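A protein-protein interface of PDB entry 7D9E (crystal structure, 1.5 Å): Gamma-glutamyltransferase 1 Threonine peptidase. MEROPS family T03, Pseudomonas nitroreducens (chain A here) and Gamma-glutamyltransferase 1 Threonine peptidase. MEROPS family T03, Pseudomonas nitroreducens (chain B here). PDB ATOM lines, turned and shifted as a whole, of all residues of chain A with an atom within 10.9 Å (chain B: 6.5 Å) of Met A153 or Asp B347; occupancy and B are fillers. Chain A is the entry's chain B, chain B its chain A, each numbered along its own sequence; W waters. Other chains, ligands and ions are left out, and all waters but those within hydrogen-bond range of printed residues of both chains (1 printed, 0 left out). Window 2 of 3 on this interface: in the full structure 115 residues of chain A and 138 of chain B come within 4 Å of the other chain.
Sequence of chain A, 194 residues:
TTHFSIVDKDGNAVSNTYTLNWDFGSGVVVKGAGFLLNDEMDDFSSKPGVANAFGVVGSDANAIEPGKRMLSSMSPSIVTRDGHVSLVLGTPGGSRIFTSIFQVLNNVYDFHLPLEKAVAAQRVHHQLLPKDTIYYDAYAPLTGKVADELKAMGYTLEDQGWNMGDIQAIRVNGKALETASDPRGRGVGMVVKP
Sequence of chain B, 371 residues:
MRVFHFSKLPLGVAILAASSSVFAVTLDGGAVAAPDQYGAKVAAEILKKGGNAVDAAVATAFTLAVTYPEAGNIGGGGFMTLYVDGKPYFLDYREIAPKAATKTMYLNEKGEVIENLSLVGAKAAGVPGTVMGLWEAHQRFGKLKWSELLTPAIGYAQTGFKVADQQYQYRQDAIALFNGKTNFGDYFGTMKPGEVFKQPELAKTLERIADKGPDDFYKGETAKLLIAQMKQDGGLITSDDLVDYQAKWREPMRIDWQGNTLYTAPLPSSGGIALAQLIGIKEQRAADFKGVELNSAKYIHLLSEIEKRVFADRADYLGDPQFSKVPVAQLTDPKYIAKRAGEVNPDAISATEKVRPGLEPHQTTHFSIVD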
ATOM      1  N   LYS A 131     -11.768  -4.798  30.249  1.00  0.00           N
ATOM      2  CA  LYS A 131     -10.671  -5.370  29.478  1.00  0.00           C
ATOM      3  C   LYS A 131     -11.140  -5.902  28.129  1.00  0.00           C
ATOM      4  O   LYS A 131     -12.069  -6.712  28.054  1.00  0.00           O
ATOM      5  CB  LYS A 131     -10.022  -6.493  30.284  1.00  0.00           C
ATOM      6  CG  LYS A 131      -8.993  -7.291  29.512  1.00  0.00           C
ATOM      7  CD  LYS A 131      -8.283  -8.302  30.413  1.00  0.00           C
ATOM      8  CE  LYS A 131      -7.253  -9.073  29.630  1.00  0.00           C
ATOM      9  NZ  LYS A 131      -6.551 -10.046  30.507  1.00  0.00           N
ATOM     10  N   ASP A 132     -10.479  -5.439  27.066  1.00  0.00           N
ATOM     11  CA  ASP A 132     -10.624  -5.999  25.718  1.00  0.00           C
ATOM     12  C   ASP A 132     -12.074  -6.059  25.261  1.00  0.00           C
ATOM     13  O   ASP A 132     -12.466  -6.937  24.489  1.00  0.00           O
ATOM     14  CB  ASP A 132      -9.953  -7.368  25.614  1.00  0.00           C
ATOM     15  CG  ASP A 132      -8.449  -7.277  25.718  1.00  0.00           C
ATOM     16  OD1 ASP A 132      -7.917  -6.164  25.524  1.00  0.00           O
ATOM     17  OD2 ASP A 132      -7.802  -8.311  25.984  1.00  0.00           O
ATOM     18  N   THR A 133     -12.876  -5.109  25.719  1.00  0.00           N
ATOM     19  CA  THR A 133     -14.292  -5.046  25.389  1.00  0.00           C
ATOM     20  C   THR A 133     -14.519  -3.930  24.381  1.00  0.00           C
ATOM     21  O   THR A 133     -14.127  -2.775  24.608  1.00  0.00           O
ATOM     22  CB  THR A 133     -15.103  -4.821  26.664  1.00  0.00           C
ATOM     23  OG1 THR A 133     -14.926  -5.948  27.533  1.00  0.00           O
ATOM     24  CG2 THR A 133     -16.577  -4.652  26.342  1.00  0.00           C
ATOM     25  N   ILE A 134     -15.114  -4.285  23.247  1.00  0.00           N
ATOM     26  CA  ILE A 134     -15.534  -3.324  22.239  1.00  0.00           C
ATOM     27  C   ILE A 134     -17.047  -3.192  22.304  1.00  0.00           C
ATOM     28  O   ILE A 134     -17.777  -4.192  22.219  1.00  0.00           O
ATOM     29  CB  ILE A 134     -15.090  -3.744  20.826  1.00  0.00           C
ATOM     30  CG1 ILE A 134     -13.569  -3.845  20.745  1.00  0.00           C
ATOM     31  CG2 ILE A 134     -15.593  -2.727  19.795  1.00  0.00           C
ATOM     32  CD1 ILE A 134     -13.065  -4.515  19.473  1.00  0.00           C
ATOM     33  N   GLY A 144     -21.179 -10.622  11.628  1.00  0.00           N
ATOM     34  CA  GLY A 144     -20.548 -11.238  10.481  1.00  0.00           C
ATOM     35  C   GLY A 144     -19.042 -11.365  10.619  1.00  0.00           C
ATOM     36  O   GLY A 144     -18.497 -11.549  11.709  1.00  0.00           O
ATOM     37  N   LYS A 145     -18.355 -11.266   9.475  1.00  0.00           N
ATOM     38  CA  LYS A 145     -16.932 -11.590   9.454  1.00  0.00           C
ATOM     39  C   LYS A 145     -16.116 -10.638  10.322  1.00  0.00           C
ATOM     40  O   LYS A 145     -15.119 -11.050  10.922  1.00  0.00           O
ATOM     41  CB  LYS A 145     -16.386 -11.597   8.023  1.00  0.00           C
ATOM     42  CG  LYS A 145     -16.451 -10.251   7.320  1.00  0.00           C
ATOM     43  CD  LYS A 145     -16.211 -10.385   5.825  1.00  0.00           C
ATOM     44  CE  LYS A 145     -16.203  -9.026   5.135  1.00  0.00           C
ATOM     45  NZ  LYS A 145     -15.541  -9.071   3.801  1.00  0.00           N
ATOM     46  N   VAL A 146     -16.502  -9.365  10.403  1.00  0.00           N
ATOM     47  CA  VAL A 146     -15.726  -8.437  11.223  1.00  0.00           C
ATOM     48  C   VAL A 146     -15.858  -8.805  12.697  1.00  0.00           C
ATOM     49  O   VAL A 146     -14.861  -8.896  13.430  1.00  0.00           O
ATOM     50  CB  VAL A 146     -16.136  -6.981  10.943  1.00  0.00           C
ATOM     51  CG1 VAL A 146     -15.458  -6.038  11.937  1.00  0.00           C
ATOM     52  CG2 VAL A 146     -15.775  -6.582   9.521  1.00  0.00           C
ATOM     53  N   ALA A 147     -17.089  -9.052  13.152  1.00  0.00           N
ATOM     54  CA  ALA A 147     -17.280  -9.480  14.531  1.00  0.00           C
ATOM     55  C   ALA A 147     -16.509 -10.759  14.815  1.00  0.00           C
ATOM     56  O   ALA A 147     -15.858 -10.884  15.856  1.00  0.00           O
ATOM     57  CB  ALA A 147     -18.770  -9.685  14.806  1.00  0.00           C
ATOM     58  N   ASP A 148     -16.569 -11.724  13.898  1.00  0.00           N
ATOM     59  CA  ASP A 148     -15.943 -13.015  14.157  1.00  0.00           C
ATOM     60  C   ASP A 148     -14.428 -12.879  14.243  1.00  0.00           C
ATOM     61  O   ASP A 148     -13.795 -13.500  15.104  1.00  0.00           O
ATOM     62  CB  ASP A 148     -16.341 -14.011  13.073  1.00  0.00           C
ATOM     63  CG  ASP A 148     -17.785 -14.473  13.203  1.00  0.00           C
ATOM     64  OD1 ASP A 148     -18.375 -14.312  14.294  1.00  0.00           O
ATOM     65  OD2 ASP A 148     -18.325 -15.010  12.216  1.00  0.00           O
ATOM     66  N   GLU A 149     -13.833 -12.072  13.363  1.00  0.00           N
ATOM     67  CA  GLU A 149     -12.394 -11.877  13.442  1.00  0.00           C
ATOM     68  C   GLU A 149     -12.003 -11.174  14.736  1.00  0.00           C
ATOM     69  O   GLU A 149     -11.025 -11.561  15.387  1.00  0.00           O
ATOM     70  CB  GLU A 149     -11.858 -11.093  12.253  1.00  0.00           C
ATOM     71  CG  GLU A 149     -10.328 -11.085  12.300  1.00  0.00           C
ATOM     72  CD  GLU A 149      -9.673 -10.559  11.053  1.00  0.00           C
ATOM     73  OE1 GLU A 149     -10.364 -10.459  10.020  1.00  0.00           O
ATOM     74  OE2 GLU A 149      -8.462 -10.261  11.109  1.00  0.00           O
ATOM     75  N   LEU A 150     -12.741 -10.133  15.122  1.00  0.00           N
ATOM     76  CA  LEU A 150     -12.407  -9.446  16.365  1.00  0.00           C
ATOM     77  C   LEU A 150     -12.479 -10.408  17.544  1.00  0.00           C
ATOM     78  O   LEU A 150     -11.616 -10.385  18.426  1.00  0.00           O
ATOM     79  CB  LEU A 150     -13.325  -8.255  16.596  1.00  0.00           C
ATOM     80  CG  LEU A 150     -13.153  -7.077  15.656  1.00  0.00           C
ATOM     81  CD1 LEU A 150     -14.297  -6.101  15.804  1.00  0.00           C
ATOM     82  CD2 LEU A 150     -11.809  -6.390  15.900  1.00  0.00           C
ATOM     83  N   LYS A 151     -13.502 -11.267  17.572  1.00  0.00           N
ATOM     84  CA  LYS A 151     -13.592 -12.258  18.641  1.00  0.00           C
ATOM     85  C   LYS A 151     -12.416 -13.226  18.585  1.00  0.00           C
ATOM     86  O   LYS A 151     -11.877 -13.619  19.629  1.00  0.00           O
ATOM     87  CB  LYS A 151     -14.921 -13.003  18.559  1.00  0.00           C
ATOM     88  CG  LYS A 151     -16.116 -12.135  18.957  1.00  0.00           C
ATOM     89  CD  LYS A 151     -17.359 -12.973  19.234  1.00  0.00           C
ATOM     90  CE  LYS A 151     -18.464 -12.682  18.255  1.00  0.00           C
ATOM     91  NZ  LYS A 151     -19.797 -13.054  18.824  1.00  0.00           N
ATOM     92  N   ALA A 152     -11.979 -13.587  17.375  1.00  0.00           N
ATOM     93  CA  ALA A 152     -10.812 -14.457  17.225  1.00  0.00           C
ATOM     94  C   ALA A 152      -9.534 -13.802  17.744  1.00  0.00           C
ATOM     95  O   ALA A 152      -8.647 -14.504  18.251  1.00  0.00           O
ATOM     96  CB  ALA A 152     -10.646 -14.857  15.757  1.00  0.00           C
ATOM     97  N   MET A 153      -9.406 -12.474  17.610  1.00  0.00           N
ATOM     98  CA  MET A 153      -8.264 -11.775  18.199  1.00  0.00           C
ATOM     99  C   MET A 153      -8.293 -11.790  19.725  1.00  0.00           C
ATOM    100  O   MET A 153      -7.240 -11.608  20.357  1.00  0.00           O
ATOM    101  CB  MET A 153      -8.176 -10.312  17.743  1.00  0.00           C
ATOM    102  CG  MET A 153      -8.273 -10.063  16.247  1.00  0.00           C
ATOM    103  SD  MET A 153      -7.729  -8.415  15.745  1.00  0.00           S
ATOM    104  CE  MET A 153      -6.029  -8.411  16.302  1.00  0.00           C
ATOM    105  N   GLY A 154      -9.471 -11.978  20.327  1.00  0.00           N
ATOM    106  CA  GLY A 154      -9.617 -12.038  21.767  1.00  0.00           C
ATOM    107  C   GLY A 154     -10.492 -10.950  22.364  1.00  0.00           C
ATOM    108  O   GLY A 154     -10.529 -10.785  23.589  1.00  0.00           O
ATOM    109  N   TYR A 155     -11.198 -10.200  21.524  1.00  0.00           N
ATOM    110  CA  TYR A 155     -12.085  -9.160  22.018  1.00  0.00           C
ATOM    111  C   TYR A 155     -13.429  -9.726  22.461  1.00  0.00           C
ATOM    112  O   TYR A 155     -13.936 -10.707  21.902  1.00  0.00           O
ATOM    113  CB  TYR A 155     -12.362  -8.132  20.923  1.00  0.00           C
ATOM    114  CG  TYR A 155     -11.203  -7.219  20.602  1.00  0.00           C
ATOM    115  CD1 TYR A 155     -10.809  -6.221  21.483  1.00  0.00           C
ATOM    116  CD2 TYR A 155     -10.511  -7.336  19.405  1.00  0.00           C
ATOM    117  CE1 TYR A 155      -9.766  -5.381  21.175  1.00  0.00           C
ATOM    118  CE2 TYR A 155      -9.473  -6.506  19.091  1.00  0.00           C
ATOM    119  CZ  TYR A 155      -9.098  -5.522  19.984  1.00  0.00           C
ATOM    120  OH  TYR A 155      -8.065  -4.666  19.692  1.00  0.00           O
ATOM    121  N   THR A 156     -14.007  -9.089  23.477  1.00  0.00           N
ATOM    122  CA  THR A 156     -15.400  -9.285  23.861  1.00  0.00           C
ATOM    123  C   THR A 156     -16.200  -8.157  23.229  1.00  0.00           C
ATOM    124  O   THR A 156     -15.811  -6.990  23.338  1.00  0.00           O
ATOM    125  CB  THR A 156     -15.553  -9.230  25.381  1.00  0.00           C
ATOM    126  OG1 THR A 156     -14.841 -10.322  25.983  1.00  0.00           O
ATOM    127  CG2 THR A 156     -17.016  -9.299  25.784  1.00  0.00           C
ATOM    128  N   LEU A 157     -17.289  -8.497  22.545  1.00  0.00           N
ATOM    129  CA  LEU A 157     -18.138  -7.506  21.897  1.00  0.00           C
ATOM    130  C   LEU A 157     -19.439  -7.394  22.676  1.00  0.00           C
ATOM    131  O   LEU A 157     -20.097  -8.411  22.932  1.00  0.00           O
ATOM    132  CB  LEU A 157     -18.450  -7.904  20.455  1.00  0.00           C
ATOM    133  CG  LEU A 157     -17.246  -8.350  19.627  1.00  0.00           C
ATOM    134  CD1 LEU A 157     -17.683  -8.671  18.212  1.00  0.00           C
ATOM    135  CD2 LEU A 157     -16.157  -7.311  19.613  1.00  0.00           C
ATOM    136  N   ALA B 297     -12.059  -5.500  10.562  1.00  0.00           N
ATOM    137  CA  ALA B 297     -11.525  -5.926  11.848  1.00  0.00           C
ATOM    138  C   ALA B 297     -10.188  -5.252  12.133  1.00  0.00           C
ATOM    139  O   ALA B 297      -9.948  -4.779  13.248  1.00  0.00           O
ATOM    140  CB  ALA B 297     -11.383  -7.447  11.889  1.00  0.00           C
ATOM    141  N   LYS B 298      -9.304  -5.184  11.136  1.00  0.00           N
ATOM    142  CA  LYS B 298      -8.002  -4.566  11.359  1.00  0.00           C
ATOM    143  C   LYS B 298      -8.150  -3.098  11.741  1.00  0.00           C
ATOM    144  O   LYS B 298      -7.465  -2.616  12.656  1.00  0.00           O
ATOM    145  CB  LYS B 298      -7.119  -4.737  10.124  1.00  0.00           C
ATOM    146  CG  LYS B 298      -5.793  -3.993  10.203  1.00  0.00           C
ATOM    147  CD  LYS B 298      -4.851  -4.667  11.169  1.00  0.00           C
ATOM    148  N   HIS B 301      -9.445  -2.890  15.292  1.00  0.00           N
ATOM    149  CA  HIS B 301      -8.387  -3.290  16.208  1.00  0.00           C
ATOM    150  C   HIS B 301      -7.374  -2.167  16.385  1.00  0.00           C
ATOM    151  O   HIS B 301      -6.952  -1.870  17.506  1.00  0.00           O
ATOM    152  CB  HIS B 301      -7.694  -4.547  15.690  1.00  0.00           C
ATOM    153  CG  HIS B 301      -6.414  -4.825  16.393  1.00  0.00           C
ATOM    154  ND1 HIS B 301      -6.368  -5.143  17.733  1.00  0.00           N
ATOM    155  CD2 HIS B 301      -5.132  -4.782  15.967  1.00  0.00           C
ATOM    156  CE1 HIS B 301      -5.108  -5.307  18.094  1.00  0.00           C
ATOM    157  NE2 HIS B 301      -4.341  -5.096  17.041  1.00  0.00           N
ATOM    158  N   LEU B 302      -6.974  -1.529  15.285  1.00  0.00           N
ATOM    159  CA  LEU B 302      -6.023  -0.424  15.374  1.00  0.00           C
ATOM    160  C   LEU B 302      -6.576   0.705  16.229  1.00  0.00           C
ATOM    161  O   LEU B 302      -5.877   1.222  17.106  1.00  0.00           O
ATOM    162  CB  LEU B 302      -5.674   0.075  13.976  1.00  0.00           C
ATOM    163  CG  LEU B 302      -4.724  -0.795  13.145  1.00  0.00           C
ATOM    164  CD1 LEU B 302      -4.652  -0.289  11.710  1.00  0.00           C
ATOM    165  CD2 LEU B 302      -3.344  -0.819  13.780  1.00  0.00           C
ATOM    166  N   VAL B 344       1.510   0.708  19.762  1.00  0.00           N
ATOM    167  CA  VAL B 344       0.384   0.112  19.061  1.00  0.00           C
ATOM    168  C   VAL B 344       0.825  -1.177  18.385  1.00  0.00           C
ATOM    169  O   VAL B 344       1.819  -1.211  17.646  1.00  0.00           O
ATOM    170  CB  VAL B 344      -0.178   1.112  18.042  1.00  0.00           C
ATOM    171  CG1 VAL B 344      -1.139   0.418  17.071  1.00  0.00           C
ATOM    172  CG2 VAL B 344      -0.874   2.254  18.766  1.00  0.00           C
ATOM    173  N   ASN B 345       0.070  -2.246  18.625  1.00  0.00           N
ATOM    174  CA  ASN B 345       0.359  -3.533  18.019  1.00  0.00           C
ATOM    175  C   ASN B 345      -0.630  -3.764  16.885  1.00  0.00           C
ATOM    176  O   ASN B 345      -1.828  -3.984  17.150  1.00  0.00           O
ATOM    177  CB  ASN B 345       0.256  -4.637  19.069  1.00  0.00           C
ATOM    178  CG  ASN B 345       0.704  -5.982  18.545  1.00  0.00           C
ATOM    179  OD1 ASN B 345       0.648  -6.239  17.345  1.00  0.00           O
ATOM    180  ND2 ASN B 345       1.197  -6.836  19.442  1.00  0.00           N
ATOM    181  N   PRO B 346      -0.197  -3.708  15.621  1.00  0.00           N
ATOM    182  CA  PRO B 346      -1.158  -3.773  14.513  1.00  0.00           C
ATOM    183  C   PRO B 346      -1.730  -5.156  14.287  1.00  0.00           C
ATOM    184  O   PRO B 346      -2.706  -5.279  13.542  1.00  0.00           O
ATOM    185  CB  PRO B 346      -0.319  -3.370  13.285  1.00  0.00           C
ATOM    186  CG  PRO B 346       0.896  -2.732  13.837  1.00  0.00           C
ATOM    187  CD  PRO B 346       1.168  -3.519  15.097  1.00  0.00           C
ATOM    188  N   ASP B 347      -1.134  -6.192  14.880  1.00  0.00           N
ATOM    189  CA  ASP B 347      -1.480  -7.568  14.555  1.00  0.00           C
ATOM    190  C   ASP B 347      -2.111  -8.341  15.706  1.00  0.00           C
ATOM    191  O   ASP B 347      -2.716  -9.386  15.459  1.00  0.00           O
ATOM    192  CB  ASP B 347      -0.229  -8.306  14.048  1.00  0.00           C
ATOM    193  CG  ASP B 347       0.470  -7.565  12.905  1.00  0.00           C
ATOM    194  N   ALA B 348      -2.019  -7.845  16.939  1.00  0.00           N
ATOM    195  CA  ALA B 348      -2.546  -8.548  18.101  1.00  0.00           C
ATOM    196  C   ALA B 348      -2.894  -7.557  19.204  1.00  0.00           C
ATOM    197  O   ALA B 348      -2.418  -6.422  19.223  1.00  0.00           O
ATOM    198  CB  ALA B 348      -1.539  -9.578  18.634  1.00  0.00           C
ATOM    199  N   ILE B 349      -3.730  -8.013  20.139  1.00  0.00           N
ATOM    200  CA  ILE B 349      -4.141  -7.180  21.260  1.00  0.00           C
ATOM    201  C   ILE B 349      -2.995  -7.071  22.256  1.00  0.00           C
ATOM    202  O   ILE B 349      -2.448  -8.083  22.714  1.00  0.00           O
ATOM    203  CB  ILE B 349      -5.372  -7.784  21.945  1.00  0.00           C
ATOM    204  CG1 ILE B 349      -6.562  -7.843  20.975  1.00  0.00           C
ATOM    205  CG2 ILE B 349      -5.748  -6.962  23.163  1.00  0.00           C
ATOM    206  CD1 ILE B 349      -7.758  -8.587  21.551  1.00  0.00           C
HETATM  207  O   HOH W   1      -4.849 -10.668  19.614  1.00  0.00           O
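The side-chain amide oxygen of Asn B345 lies within hydrogen-bond range of the backbone NH of Asp B347. The backbone carbonyl oxygen (O) of Asp A132 is in hydrogen-bond range of the backbone NH (N) of Thr A156, at 2.8 Å. The backbone NH (N) of Ala B348 lies within hydrogen-bond range of the side-chain amide oxygen (OD1) of Asn B345. O of Ala B348 sits close to NE2 of His B301. O of Leu A150 is in hydrogen-bond range of N of Tyr A155. The backbone carbonyl oxygen (O) of Asn B345 is in hydrogen-bond range of a ring nitrogen (NE2) of His B301 (2.8 Å).
Water W1 bridges O of Met A153 and N of Ile B349.
A ring nitrogen (ND1) of His B301 sits at hydrogen-bond distance from the side-chain hydroxyl (OH) of Tyr A155, 2.6 Å away.
Hydrophobic or aromatic side chains of chain A within 4 Å of the printed part of chain B: Val A146, Leu A150, Met A153 and Tyr A155. Printed residues of chain B that touch a printed residue of chain A: Ala B297, His B301, Asp B347, Ala B348 and Ile B349. Along chain B the printed residues that touch a printed residue of chain A span positions 297 to 349. Among the printed residues, 11 pairs touch across the chains. Among the printed residues, no Asp or Glu carboxylate lies within 4 Å of a Lys or Arg side-chain nitrogen of the other chain.
Among the printed residues, pairs that only touch across the chains: Met A153 with Ile B349 (3.3 Å), Asp A132 with Ile B349 (3.3 Å), Met A153 with Asp B347 (3.6 Å), Tyr A155 with Ile B349 (3.6 Å), Met A153 with His B301 (3.6 Å), Leu A150 with Ala B297 (3.6 Å), Glu A149 with Ala B297 (3.6 Å), Gly A154 with Ile B349 (3.7 Å), Val A146 with Ala B297 (3.7 Å) and Met A153 with Ala B348 (3.9 Å).
Met A153 touches just these residues of chain B: His B301, Asp B347, Ala B348 and Ile B349. Of chain A, only Met A153 comes within 4 Å of Asp B347. His B301 touches just these residues of chain A: Met A153 and Tyr A155. Pro B346 touches none of the printed residues of chain A. Printed residues of chain B within 4 Å of Gly A154: Ile B349. Of the printed residues of chain B, Asp A132 touches Ile B349. Of the printed residues of chain B, Val A146 touches Ala B297 (3.7 Å). Of the printed residues of chain B, Glu A149 touches Ala B297 (3.6 Å). Printed residues of chain B within 4 Å of Tyr A155: His B301 (2.6 Å) and Ile B349 (3.6 Å). Gly A144 touches none of the printed residues of chain B. Val B344 touches none of the printed residues of chain A. The nearest printed residue of chain B that does not touch Asp A132 is His B301 (8.0 Å).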
